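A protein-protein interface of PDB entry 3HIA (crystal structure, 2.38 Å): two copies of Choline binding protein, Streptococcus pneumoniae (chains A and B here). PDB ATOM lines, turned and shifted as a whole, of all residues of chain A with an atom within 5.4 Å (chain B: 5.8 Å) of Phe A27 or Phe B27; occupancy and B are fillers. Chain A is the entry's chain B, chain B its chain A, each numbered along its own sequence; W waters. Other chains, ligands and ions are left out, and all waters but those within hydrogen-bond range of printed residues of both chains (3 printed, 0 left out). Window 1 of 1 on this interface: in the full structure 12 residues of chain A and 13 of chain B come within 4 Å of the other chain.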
ATOM      1  N   GLY A  17     -25.264   2.829  12.498  1.00  0.00           N
ATOM      2  CA  GLY A  17     -26.634   3.147  12.899  1.00  0.00           C
ATOM      3  C   GLY A  17     -26.820   3.224  14.398  1.00  0.00           C
ATOM      4  O   GLY A  17     -25.929   3.683  15.124  1.00  0.00           O
ATOM      5  N   TRP A  18     -27.978   2.757  14.865  1.00  0.00           N
ATOM      6  CA  TRP A  18     -28.342   2.862  16.289  1.00  0.00           C
ATOM      7  C   TRP A  18     -27.621   1.845  17.146  1.00  0.00           C
ATOM      8  O   TRP A  18     -27.656   0.648  16.865  1.00  0.00           O
ATOM      9  CB  TRP A  18     -29.851   2.706  16.508  1.00  0.00           C
ATOM     10  CG  TRP A  18     -30.680   3.755  15.846  1.00  0.00           C
ATOM     11  CD1 TRP A  18     -31.544   3.577  14.815  1.00  0.00           C
ATOM     12  CD2 TRP A  18     -30.716   5.144  16.169  1.00  0.00           C
ATOM     13  NE1 TRP A  18     -32.120   4.770  14.468  1.00  0.00           N
ATOM     14  CE2 TRP A  18     -31.631   5.750  15.289  1.00  0.00           C
ATOM     15  CE3 TRP A  18     -30.069   5.936  17.134  1.00  0.00           C
ATOM     16  CZ2 TRP A  18     -31.924   7.113  15.332  1.00  0.00           C
ATOM     17  CZ3 TRP A  18     -30.348   7.292  17.178  1.00  0.00           C
ATOM     18  CH2 TRP A  18     -31.273   7.870  16.280  1.00  0.00           C
ATOM     19  N   LYS A  19     -26.985   2.333  18.202  1.00  0.00           N
ATOM     20  CA  LYS A  19     -26.305   1.486  19.165  1.00  0.00           C
ATOM     21  C   LYS A  19     -26.605   2.047  20.546  1.00  0.00           C
ATOM     22  O   LYS A  19     -26.536   3.262  20.746  1.00  0.00           O
ATOM     23  CB  LYS A  19     -24.802   1.512  18.896  1.00  0.00           C
ATOM     24  CG  LYS A  19     -24.010   0.441  19.626  1.00  0.00           C
ATOM     25  CD  LYS A  19     -22.559   0.448  19.206  1.00  0.00           C
ATOM     26  CE  LYS A  19     -21.713  -0.282  20.218  1.00  0.00           C
ATOM     27  NZ  LYS A  19     -22.081  -1.727  20.316  1.00  0.00           N
ATOM     28  N   TRP A  25     -28.790   5.866  23.632  1.00  0.00           N
ATOM     29  CA  TRP A  25     -28.668   5.540  22.222  1.00  0.00           C
ATOM     30  C   TRP A  25     -27.759   6.500  21.474  1.00  0.00           C
ATOM     31  O   TRP A  25     -27.787   7.722  21.705  1.00  0.00           O
ATOM     32  CB  TRP A  25     -30.034   5.529  21.558  1.00  0.00           C
ATOM     33  CG  TRP A  25     -30.854   4.364  21.955  1.00  0.00           C
ATOM     34  CD1 TRP A  25     -31.772   4.315  22.966  1.00  0.00           C
ATOM     35  CD2 TRP A  25     -30.831   3.056  21.365  1.00  0.00           C
ATOM     36  NE1 TRP A  25     -32.329   3.065  23.034  1.00  0.00           N
ATOM     37  CE2 TRP A  25     -31.769   2.269  22.065  1.00  0.00           C
ATOM     38  CE3 TRP A  25     -30.110   2.476  20.314  1.00  0.00           C
ATOM     39  CZ2 TRP A  25     -32.015   0.931  21.743  1.00  0.00           C
ATOM     40  CZ3 TRP A  25     -30.350   1.141  19.999  1.00  0.00           C
ATOM     41  CH2 TRP A  25     -31.295   0.387  20.710  1.00  0.00           C
ATOM     42  N   TYR A  26     -26.966   5.917  20.570  1.00  0.00           N
ATOM     43  CA  TYR A  26     -26.038   6.642  19.715  1.00  0.00           C
ATOM     44  C   TYR A  26     -26.286   6.227  18.275  1.00  0.00           C
ATOM     45  O   TYR A  26     -26.801   5.125  18.020  1.00  0.00           O
ATOM     46  CB  TYR A  26     -24.591   6.331  20.119  1.00  0.00           C
ATOM     47  CG  TYR A  26     -24.286   6.669  21.566  1.00  0.00           C
ATOM     48  CD1 TYR A  26     -24.580   5.767  22.593  1.00  0.00           C
ATOM     49  CD2 TYR A  26     -23.707   7.896  21.908  1.00  0.00           C
ATOM     50  CE1 TYR A  26     -24.309   6.086  23.939  1.00  0.00           C
ATOM     51  CE2 TYR A  26     -23.440   8.230  23.238  1.00  0.00           C
ATOM     52  CZ  TYR A  26     -23.744   7.324  24.247  1.00  0.00           C
ATOM     53  OH  TYR A  26     -23.472   7.648  25.557  1.00  0.00           O
ATOM     54  N   PHE A  27     -25.933   7.110  17.338  1.00  0.00           N
ATOM     55  CA  PHE A  27     -26.026   6.796  15.911  1.00  0.00           C
ATOM     56  C   PHE A  27     -24.629   6.799  15.302  1.00  0.00           C
ATOM     57  O   PHE A  27     -23.902   7.786  15.380  1.00  0.00           O
ATOM     58  CB  PHE A  27     -26.962   7.775  15.184  1.00  0.00           C
ATOM     59  CG  PHE A  27     -27.392   7.314  13.820  1.00  0.00           C
ATOM     60  CD1 PHE A  27     -28.669   6.790  13.625  1.00  0.00           C
ATOM     61  CD2 PHE A  27     -26.530   7.421  12.718  1.00  0.00           C
ATOM     62  CE1 PHE A  27     -29.087   6.367  12.353  1.00  0.00           C
ATOM     63  CE2 PHE A  27     -26.927   7.006  11.439  1.00  0.00           C
ATOM     64  CZ  PHE A  27     -28.208   6.473  11.254  1.00  0.00           C
ATOM     65  N   TYR A  28     -24.256   5.673  14.713  1.00  0.00           N
ATOM     66  CA  TYR A  28     -22.919   5.498  14.175  1.00  0.00           C
ATOM     67  C   TYR A  28     -22.857   5.621  12.651  1.00  0.00           C
ATOM     68  O   TYR A  28     -23.605   4.962  11.928  1.00  0.00           O
ATOM     69  CB  TYR A  28     -22.340   4.158  14.648  1.00  0.00           C
ATOM     70  CG  TYR A  28     -21.769   4.246  16.033  1.00  0.00           C
ATOM     71  CD1 TYR A  28     -22.589   4.140  17.154  1.00  0.00           C
ATOM     72  CD2 TYR A  28     -20.411   4.473  16.224  1.00  0.00           C
ATOM     73  CE1 TYR A  28     -22.060   4.233  18.446  1.00  0.00           C
ATOM     74  CE2 TYR A  28     -19.865   4.563  17.503  1.00  0.00           C
ATOM     75  CZ  TYR A  28     -20.693   4.445  18.611  1.00  0.00           C
ATOM     76  OH  TYR A  28     -20.148   4.540  19.881  1.00  0.00           O
ATOM     77  N   ASN A  29     -21.950   6.478  12.185  1.00  0.00           N
ATOM     78  CA  ASN A  29     -21.716   6.670  10.760  1.00  0.00           C
ATOM     79  C   ASN A  29     -20.790   5.596  10.203  1.00  0.00           C
ATOM     80  O   ASN A  29     -20.046   4.955  10.959  1.00  0.00           O
ATOM     81  CB  ASN A  29     -21.148   8.068  10.494  1.00  0.00           C
ATOM     82  CG  ASN A  29     -22.153   9.171  10.782  1.00  0.00           C
ATOM     83  OD1 ASN A  29     -23.302   9.115  10.336  1.00  0.00           O
ATOM     84  ND2 ASN A  29     -21.721  10.188  11.519  1.00  0.00           N
ATOM     85  N   SER A  33     -17.585   7.696  12.930  1.00  0.00           N
ATOM     86  CA  SER A  33     -17.888   8.842  13.767  1.00  0.00           C
ATOM     87  C   SER A  33     -19.331   8.742  14.226  1.00  0.00           C
ATOM     88  O   SER A  33     -20.118   8.041  13.601  1.00  0.00           O
ATOM     89  CB  SER A  33     -17.638  10.137  12.995  1.00  0.00           C
ATOM     90  OG  SER A  33     -18.491  10.240  11.874  1.00  0.00           O
ATOM     91  N   MET A  34     -19.671   9.407  15.328  1.00  0.00           N
ATOM     92  CA  MET A  34     -21.061   9.444  15.797  1.00  0.00           C
ATOM     93  C   MET A  34     -21.765  10.670  15.236  1.00  0.00           C
ATOM     94  O   MET A  34     -21.184  11.772  15.183  1.00  0.00           O
ATOM     95  CB  MET A  34     -21.160   9.523  17.323  1.00  0.00           C
ATOM     96  CG  MET A  34     -20.652   8.329  18.110  1.00  0.00           C
ATOM     97  SD  MET A  34     -20.411   8.743  19.861  1.00  0.00           S
ATOM     98  CE  MET A  34     -18.958   9.788  19.783  1.00  0.00           C
ATOM     99  N   ALA A  35     -23.022  10.474  14.845  1.00  0.00           N
ATOM    100  CA  ALA A  35     -23.889  11.540  14.382  1.00  0.00           C
ATOM    101  C   ALA A  35     -24.332  12.425  15.544  1.00  0.00           C
ATOM    102  O   ALA A  35     -24.579  11.937  16.645  1.00  0.00           O
ATOM    103  CB  ALA A  35     -25.105  10.929  13.725  1.00  0.00           C
ATOM    104  N   VAL A  39     -31.609  13.985  13.692  1.00  0.00           N
ATOM    105  CA  VAL A  39     -31.625  12.799  12.833  1.00  0.00           C
ATOM    106  C   VAL A  39     -33.065  12.489  12.458  1.00  0.00           C
ATOM    107  O   VAL A  39     -33.951  12.410  13.323  1.00  0.00           O
ATOM    108  CB  VAL A  39     -30.921  11.584  13.497  1.00  0.00           C
ATOM    109  CG1 VAL A  39     -31.079  10.308  12.662  1.00  0.00           C
ATOM    110  CG2 VAL A  39     -29.455  11.864  13.652  1.00  0.00           C
ATOM    111  N   VAL A  41     -35.104   9.453  10.636  1.00  0.00           N
ATOM    112  CA  VAL A  41     -35.076   8.111  10.085  1.00  0.00           C
ATOM    113  C   VAL A  41     -36.397   7.382  10.308  1.00  0.00           C
ATOM    114  O   VAL A  41     -36.985   7.447  11.389  1.00  0.00           O
ATOM    115  CB  VAL A  41     -33.829   7.312  10.563  1.00  0.00           C
ATOM    116  CG1 VAL A  41     -33.901   6.966  12.046  1.00  0.00           C
ATOM    117  CG2 VAL A  41     -33.597   6.090   9.687  1.00  0.00           C
ATOM    118  N   LEU A  48     -29.688  14.439  18.858  1.00  0.00           N
ATOM    119  CA  LEU A  48     -28.447  13.945  19.416  1.00  0.00           C
ATOM    120  C   LEU A  48     -27.576  15.091  19.933  1.00  0.00           C
ATOM    121  O   LEU A  48     -27.307  16.060  19.214  1.00  0.00           O
ATOM    122  CB  LEU A  48     -27.693  13.169  18.336  1.00  0.00           C
ATOM    123  CG  LEU A  48     -27.941  11.666  18.133  1.00  0.00           C
ATOM    124  CD1 LEU A  48     -29.363  11.202  18.454  1.00  0.00           C
ATOM    125  CD2 LEU A  48     -27.561  11.265  16.712  1.00  0.00           C
ATOM    126  N   GLY A  52     -23.101  12.794  21.071  1.00  0.00           N
ATOM    127  CA  GLY A  52     -23.744  11.821  20.192  1.00  0.00           C
ATOM    128  C   GLY A  52     -24.866  11.056  20.851  1.00  0.00           C
ATOM    129  O   GLY A  52     -25.497  10.201  20.219  1.00  0.00           O
ATOM    130  N   GLY B  17     -28.657  -1.206  11.297  1.00  0.00           N
ATOM    131  CA  GLY B  17     -27.889  -0.054  10.807  1.00  0.00           C
ATOM    132  C   GLY B  17     -27.746  -0.047   9.295  1.00  0.00           C
ATOM    133  O   GLY B  17     -28.447  -0.806   8.609  1.00  0.00           O
ATOM    134  N   TRP B  18     -26.855   0.813   8.781  1.00  0.00           N
ATOM    135  CA  TRP B  18     -26.509   0.845   7.352  1.00  0.00           C
ATOM    136  C   TRP B  18     -25.878  -0.473   6.905  1.00  0.00           C
ATOM    137  O   TRP B  18     -24.908  -0.968   7.503  1.00  0.00           O
ATOM    138  CB  TRP B  18     -25.538   1.979   7.014  1.00  0.00           C
ATOM    139  CG  TRP B  18     -26.072   3.361   7.198  1.00  0.00           C
ATOM    140  CD1 TRP B  18     -25.713   4.244   8.168  1.00  0.00           C
ATOM    141  CD2 TRP B  18     -27.043   4.037   6.377  1.00  0.00           C
ATOM    142  NE1 TRP B  18     -26.388   5.426   8.009  1.00  0.00           N
ATOM    143  CE2 TRP B  18     -27.220   5.327   6.924  1.00  0.00           C
ATOM    144  CE3 TRP B  18     -27.777   3.679   5.228  1.00  0.00           C
ATOM    145  CZ2 TRP B  18     -28.108   6.268   6.370  1.00  0.00           C
ATOM    146  CZ3 TRP B  18     -28.650   4.606   4.670  1.00  0.00           C
ATOM    147  CH2 TRP B  18     -28.812   5.890   5.247  1.00  0.00           C
ATOM    148  N   LYS B  19     -26.436  -1.029   5.841  1.00  0.00           N
ATOM    149  CA  LYS B  19     -25.953  -2.259   5.292  1.00  0.00           C
ATOM    150  C   LYS B  19     -25.911  -2.161   3.768  1.00  0.00           C
ATOM    151  O   LYS B  19     -26.874  -1.732   3.123  1.00  0.00           O
ATOM    152  CB  LYS B  19     -26.864  -3.400   5.732  1.00  0.00           C
ATOM    153  CG  LYS B  19     -26.122  -4.577   6.323  1.00  0.00           C
ATOM    154  CD  LYS B  19     -25.578  -4.244   7.726  1.00  0.00           C
ATOM    155  CE  LYS B  19     -24.353  -5.108   8.060  1.00  0.00           C
ATOM    156  NZ  LYS B  19     -23.780  -4.812   9.413  1.00  0.00           N
ATOM    157  N   TRP B  25     -27.242   0.464  -0.784  1.00  0.00           N
ATOM    158  CA  TRP B  25     -27.292   0.820   0.631  1.00  0.00           C
ATOM    159  C   TRP B  25     -28.708   0.725   1.161  1.00  0.00           C
ATOM    160  O   TRP B  25     -29.635   1.259   0.559  1.00  0.00           O
ATOM    161  CB  TRP B  25     -26.743   2.243   0.872  1.00  0.00           C
ATOM    162  CG  TRP B  25     -25.228   2.316   0.968  1.00  0.00           C
ATOM    163  CD1 TRP B  25     -24.372   2.860   0.055  1.00  0.00           C
ATOM    164  CD2 TRP B  25     -24.406   1.819   2.035  1.00  0.00           C
ATOM    165  NE1 TRP B  25     -23.075   2.743   0.484  1.00  0.00           N
ATOM    166  CE2 TRP B  25     -23.062   2.110   1.697  1.00  0.00           C
ATOM    167  CE3 TRP B  25     -24.676   1.171   3.247  1.00  0.00           C
ATOM    168  CZ2 TRP B  25     -21.982   1.751   2.522  1.00  0.00           C
ATOM    169  CZ3 TRP B  25     -23.605   0.829   4.073  1.00  0.00           C
ATOM    170  CH2 TRP B  25     -22.273   1.115   3.705  1.00  0.00           C
ATOM    171  N   TYR B  26     -28.849   0.023   2.288  1.00  0.00           N
ATOM    172  CA  TYR B  26     -30.108  -0.118   3.017  1.00  0.00           C
ATOM    173  C   TYR B  26     -29.880   0.316   4.448  1.00  0.00           C
ATOM    174  O   TYR B  26     -28.748   0.290   4.936  1.00  0.00           O
ATOM    175  CB  TYR B  26     -30.601  -1.569   3.005  1.00  0.00           C
ATOM    176  CG  TYR B  26     -30.862  -2.107   1.629  1.00  0.00           C
ATOM    177  CD1 TYR B  26     -29.806  -2.521   0.810  1.00  0.00           C
ATOM    178  CD2 TYR B  26     -32.163  -2.203   1.137  1.00  0.00           C
ATOM    179  CE1 TYR B  26     -30.041  -3.003  -0.469  1.00  0.00           C
ATOM    180  CE2 TYR B  26     -32.411  -2.692  -0.144  1.00  0.00           C
ATOM    181  CZ  TYR B  26     -31.345  -3.086  -0.938  1.00  0.00           C
ATOM    182  OH  TYR B  26     -31.579  -3.562  -2.209  1.00  0.00           O
ATOM    183  N   PHE B  27     -30.951   0.726   5.119  1.00  0.00           N
ATOM    184  CA  PHE B  27     -30.877   0.978   6.560  1.00  0.00           C
ATOM    185  C   PHE B  27     -31.803   0.074   7.339  1.00  0.00           C
ATOM    186  O   PHE B  27     -32.990   0.010   7.066  1.00  0.00           O
ATOM    187  CB  PHE B  27     -31.178   2.422   6.924  1.00  0.00           C
ATOM    188  CG  PHE B  27     -30.854   2.747   8.352  1.00  0.00           C
ATOM    189  CD1 PHE B  27     -29.556   3.127   8.716  1.00  0.00           C
ATOM    190  CD2 PHE B  27     -31.843   2.678   9.342  1.00  0.00           C
ATOM    191  CE1 PHE B  27     -29.246   3.445  10.069  1.00  0.00           C
ATOM    192  CE2 PHE B  27     -31.559   2.978  10.683  1.00  0.00           C
ATOM    193  CZ  PHE B  27     -30.259   3.367  11.052  1.00  0.00           C
ATOM    194  N   TYR B  28     -31.252  -0.613   8.323  1.00  0.00           N
ATOM    195  CA  TYR B  28     -32.067  -1.484   9.149  1.00  0.00           C
ATOM    196  C   TYR B  28     -32.318  -0.861  10.514  1.00  0.00           C
ATOM    197  O   TYR B  28     -31.400  -0.326  11.155  1.00  0.00           O
ATOM    198  CB  TYR B  28     -31.429  -2.870   9.286  1.00  0.00           C
ATOM    199  CG  TYR B  28     -31.495  -3.712   8.033  1.00  0.00           C
ATOM    200  CD1 TYR B  28     -30.496  -3.636   7.060  1.00  0.00           C
ATOM    201  CD2 TYR B  28     -32.555  -4.597   7.827  1.00  0.00           C
ATOM    202  CE1 TYR B  28     -30.549  -4.402   5.906  1.00  0.00           C
ATOM    203  CE2 TYR B  28     -32.620  -5.385   6.670  1.00  0.00           C
ATOM    204  CZ  TYR B  28     -31.611  -5.282   5.716  1.00  0.00           C
ATOM    205  OH  TYR B  28     -31.681  -6.058   4.577  1.00  0.00           O
ATOM    206  N   ASN B  29     -33.586  -0.922  10.926  1.00  0.00           N
ATOM    207  CA  ASN B  29     -34.016  -0.555  12.270  1.00  0.00           C
ATOM    208  C   ASN B  29     -33.646  -1.621  13.288  1.00  0.00           C
ATOM    209  O   ASN B  29     -33.309  -2.754  12.930  1.00  0.00           O
ATOM    210  CB  ASN B  29     -35.510  -0.244  12.281  1.00  0.00           C
ATOM    211  CG  ASN B  29     -35.867   0.867  11.293  1.00  0.00           C
ATOM    212  OD1 ASN B  29     -35.252   1.939  11.297  1.00  0.00           O
ATOM    213  ND2 ASN B  29     -36.837   0.595  10.416  1.00  0.00           N
ATOM    214  N   SER B  33     -36.355  -4.273  10.895  1.00  0.00           N
ATOM    215  CA  SER B  33     -37.048  -3.757   9.701  1.00  0.00           C
ATOM    216  C   SER B  33     -36.200  -2.759   8.952  1.00  0.00           C
ATOM    217  O   SER B  33     -35.313  -2.129   9.536  1.00  0.00           O
ATOM    218  CB  SER B  33     -38.370  -3.095  10.053  1.00  0.00           C
ATOM    219  OG  SER B  33     -38.154  -2.049  10.950  1.00  0.00           O
ATOM    220  N   MET B  34     -36.481  -2.613   7.657  1.00  0.00           N
ATOM    221  CA  MET B  34     -35.818  -1.607   6.829  1.00  0.00           C
ATOM    222  C   MET B  34     -36.533  -0.275   6.934  1.00  0.00           C
ATOM    223  O   MET B  34     -37.754  -0.221   6.869  1.00  0.00           O
ATOM    224  CB  MET B  34     -35.803  -2.044   5.367  1.00  0.00           C
ATOM    225  CG  MET B  34     -35.043  -3.329   5.113  1.00  0.00           C
ATOM    226  SD  MET B  34     -34.783  -3.668   3.372  1.00  0.00           S
ATOM    227  CE  MET B  34     -36.478  -3.905   2.843  1.00  0.00           C
ATOM    228  N   ALA B  35     -35.768   0.800   7.102  1.00  0.00           N
ATOM    229  CA  ALA B  35     -36.276   2.152   6.931  1.00  0.00           C
ATOM    230  C   ALA B  35     -36.549   2.469   5.447  1.00  0.00           C
ATOM    231  O   ALA B  35     -35.897   1.946   4.553  1.00  0.00           O
ATOM    232  CB  ALA B  35     -35.286   3.157   7.514  1.00  0.00           C
ATOM    233  N   VAL B  39     -34.130  10.282   4.635  1.00  0.00           N
ATOM    234  CA  VAL B  39     -33.267  10.140   5.798  1.00  0.00           C
ATOM    235  C   VAL B  39     -32.449  11.430   5.917  1.00  0.00           C
ATOM    236  O   VAL B  39     -31.898  11.910   4.918  1.00  0.00           O
ATOM    237  CB  VAL B  39     -32.327   8.882   5.695  1.00  0.00           C
ATOM    238  CG1 VAL B  39     -31.292   8.844   6.824  1.00  0.00           C
ATOM    239  CG2 VAL B  39     -33.149   7.578   5.709  1.00  0.00           C
ATOM    240  N   VAL B  41     -29.195  12.607   8.308  1.00  0.00           N
ATOM    241  CA  VAL B  41     -28.165  12.563   9.325  1.00  0.00           C
ATOM    242  C   VAL B  41     -26.964  13.428   8.908  1.00  0.00           C
ATOM    243  O   VAL B  41     -26.683  13.579   7.704  1.00  0.00           O
ATOM    244  CB  VAL B  41     -27.730  11.140   9.566  1.00  0.00           C
ATOM    245  CG1 VAL B  41     -27.200  10.510   8.265  1.00  0.00           C
ATOM    246  CG2 VAL B  41     -26.716  11.092  10.702  1.00  0.00           C
ATOM    247  N   LEU B  48     -34.646   6.615   0.423  1.00  0.00           N
ATOM    248  CA  LEU B  48     -34.732   5.176   0.242  1.00  0.00           C
ATOM    249  C   LEU B  48     -36.045   4.821  -0.424  1.00  0.00           C
ATOM    250  O   LEU B  48     -37.130   5.238   0.002  1.00  0.00           O
ATOM    251  CB  LEU B  48     -34.590   4.440   1.568  1.00  0.00           C
ATOM    252  CG  LEU B  48     -33.520   4.896   2.563  1.00  0.00           C
ATOM    253  CD1 LEU B  48     -33.614   4.008   3.807  1.00  0.00           C
ATOM    254  CD2 LEU B  48     -32.115   4.902   2.002  1.00  0.00           C
ATOM    255  N   GLY B  52     -36.587  -0.064   0.253  1.00  0.00           N
ATOM    256  CA  GLY B  52     -35.508   0.262   1.172  1.00  0.00           C
ATOM    257  C   GLY B  52     -34.173   0.638   0.567  1.00  0.00           C
ATOM    258  O   GLY B  52     -33.279   1.047   1.299  1.00  0.00           O
HETATM  259  O   HOH W   1     -27.742  -0.663  14.496  1.00  0.00           O
HETATM  260  O   HOH W   2     -30.137   0.729  13.194  1.00  0.00           O
HETATM  261  O   HOH W   3     -25.011   7.827   8.466  1.00  0.00           O
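The backbone carbonyl oxygen of Gly A17 lies within hydrogen-bond range of the backbone NH of Tyr A28, 2.6 Å away. The backbone NH (N) of Ala A35 lies within hydrogen-bond range of the backbone carbonyl oxygen (O) of Phe A27 (2.9 Å). The backbone NH (N) of Ala B35 lies within hydrogen-bond range of the backbone carbonyl oxygen (O) of Phe B27, at 2.9 Å. ND2 of Asn A29 is in hydrogen-bond range of OG of Ser A33 (3.2 Å).
CA of Gly A17 touches CE1 of Phe B27, at 3.9 Å. Trp A18 touches Phe B27. CE2 of Phe A27 touches NE1 of Trp B18, at 3.8 Å. CZ of Phe A27 touches CE1 of Phe B27, at 3.4 Å. OD1 of Asn A29 touches CG2 of Val B41, 3.96 Å away. Val B41 touches Ala A35 (CG2 to CB, 3.4 Å). Val A41 touches Phe B27.
Phe A27 touches two residues of chain B. Printed residues of chain A within 4 Å of Phe B27: Gly A17, Trp A18, Phe A27 and Val A41. Printed residues of chain A within 4 Å of Val B41: Asn A29 (3.96 Å) and Ala A35 (3.4 Å). Printed residues of chain B within 4 Å of Gly A17: Phe B27 (3.9 Å). Trp A25 touches none of the printed residues of chain B. The nearest printed residue of chain A that does not touch Phe B27 is Tyr A28 (6.1 Å).
Of the 15 printed residues of chain B, 3 touch a printed residue of chain A. Printed residues of chain A that touch a printed residue of chain B: Gly A17, Trp A18, Phe A27, Asn A29, Ala A35 and Val A41. Hydrophobic or aromatic side chains of chain A within 4 Å of the printed part of chain B: Trp A18, Phe A27, Ala A35 and Val A41. Among the printed residues, 7 pairs touch across the chains. Among the printed residues, no Asp or Glu carboxylate lies within 4 Å of a Lys or Arg side-chain nitrogen of the other chain.
Trp A18 touches Phe B27, and with the chains exchanged Phe A27 touches Trp B18. Asn A29 touches Val B41, but with the chains exchanged Val A41 does not touch Asn B29 (4.7 Å). Ala A35 touches Val B41, but with the chains exchanged Val A41 does not touch Ala B35 (4.02 Å). Val A41 touches Phe B27, but with the chains exchanged Phe A27 does not touch Val B41 (4.2 Å). Positions printed for both chains: 17, 18, 19, 25, 26, 27, 28, 29, 33, 34, 35, 39, 41, 48 and 52.
Water W2 lies within hydrogen-bond range of O of Tyr B28 (2.6 Å), N of Gly B17 (3.1 Å) and N of Trp A18 (3.4 Å). Water W1 bridges the backbone carbonyl oxygen of Trp A18 (2.7 Å) and the backbone NH of Gly B17 (3.4 Å). Water W3 bridges the indole nitrogen (NE1) of Trp B18 (2.8 Å) and the side-chain amide oxygen (OD1) of Asn A29 (2.8 Å).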
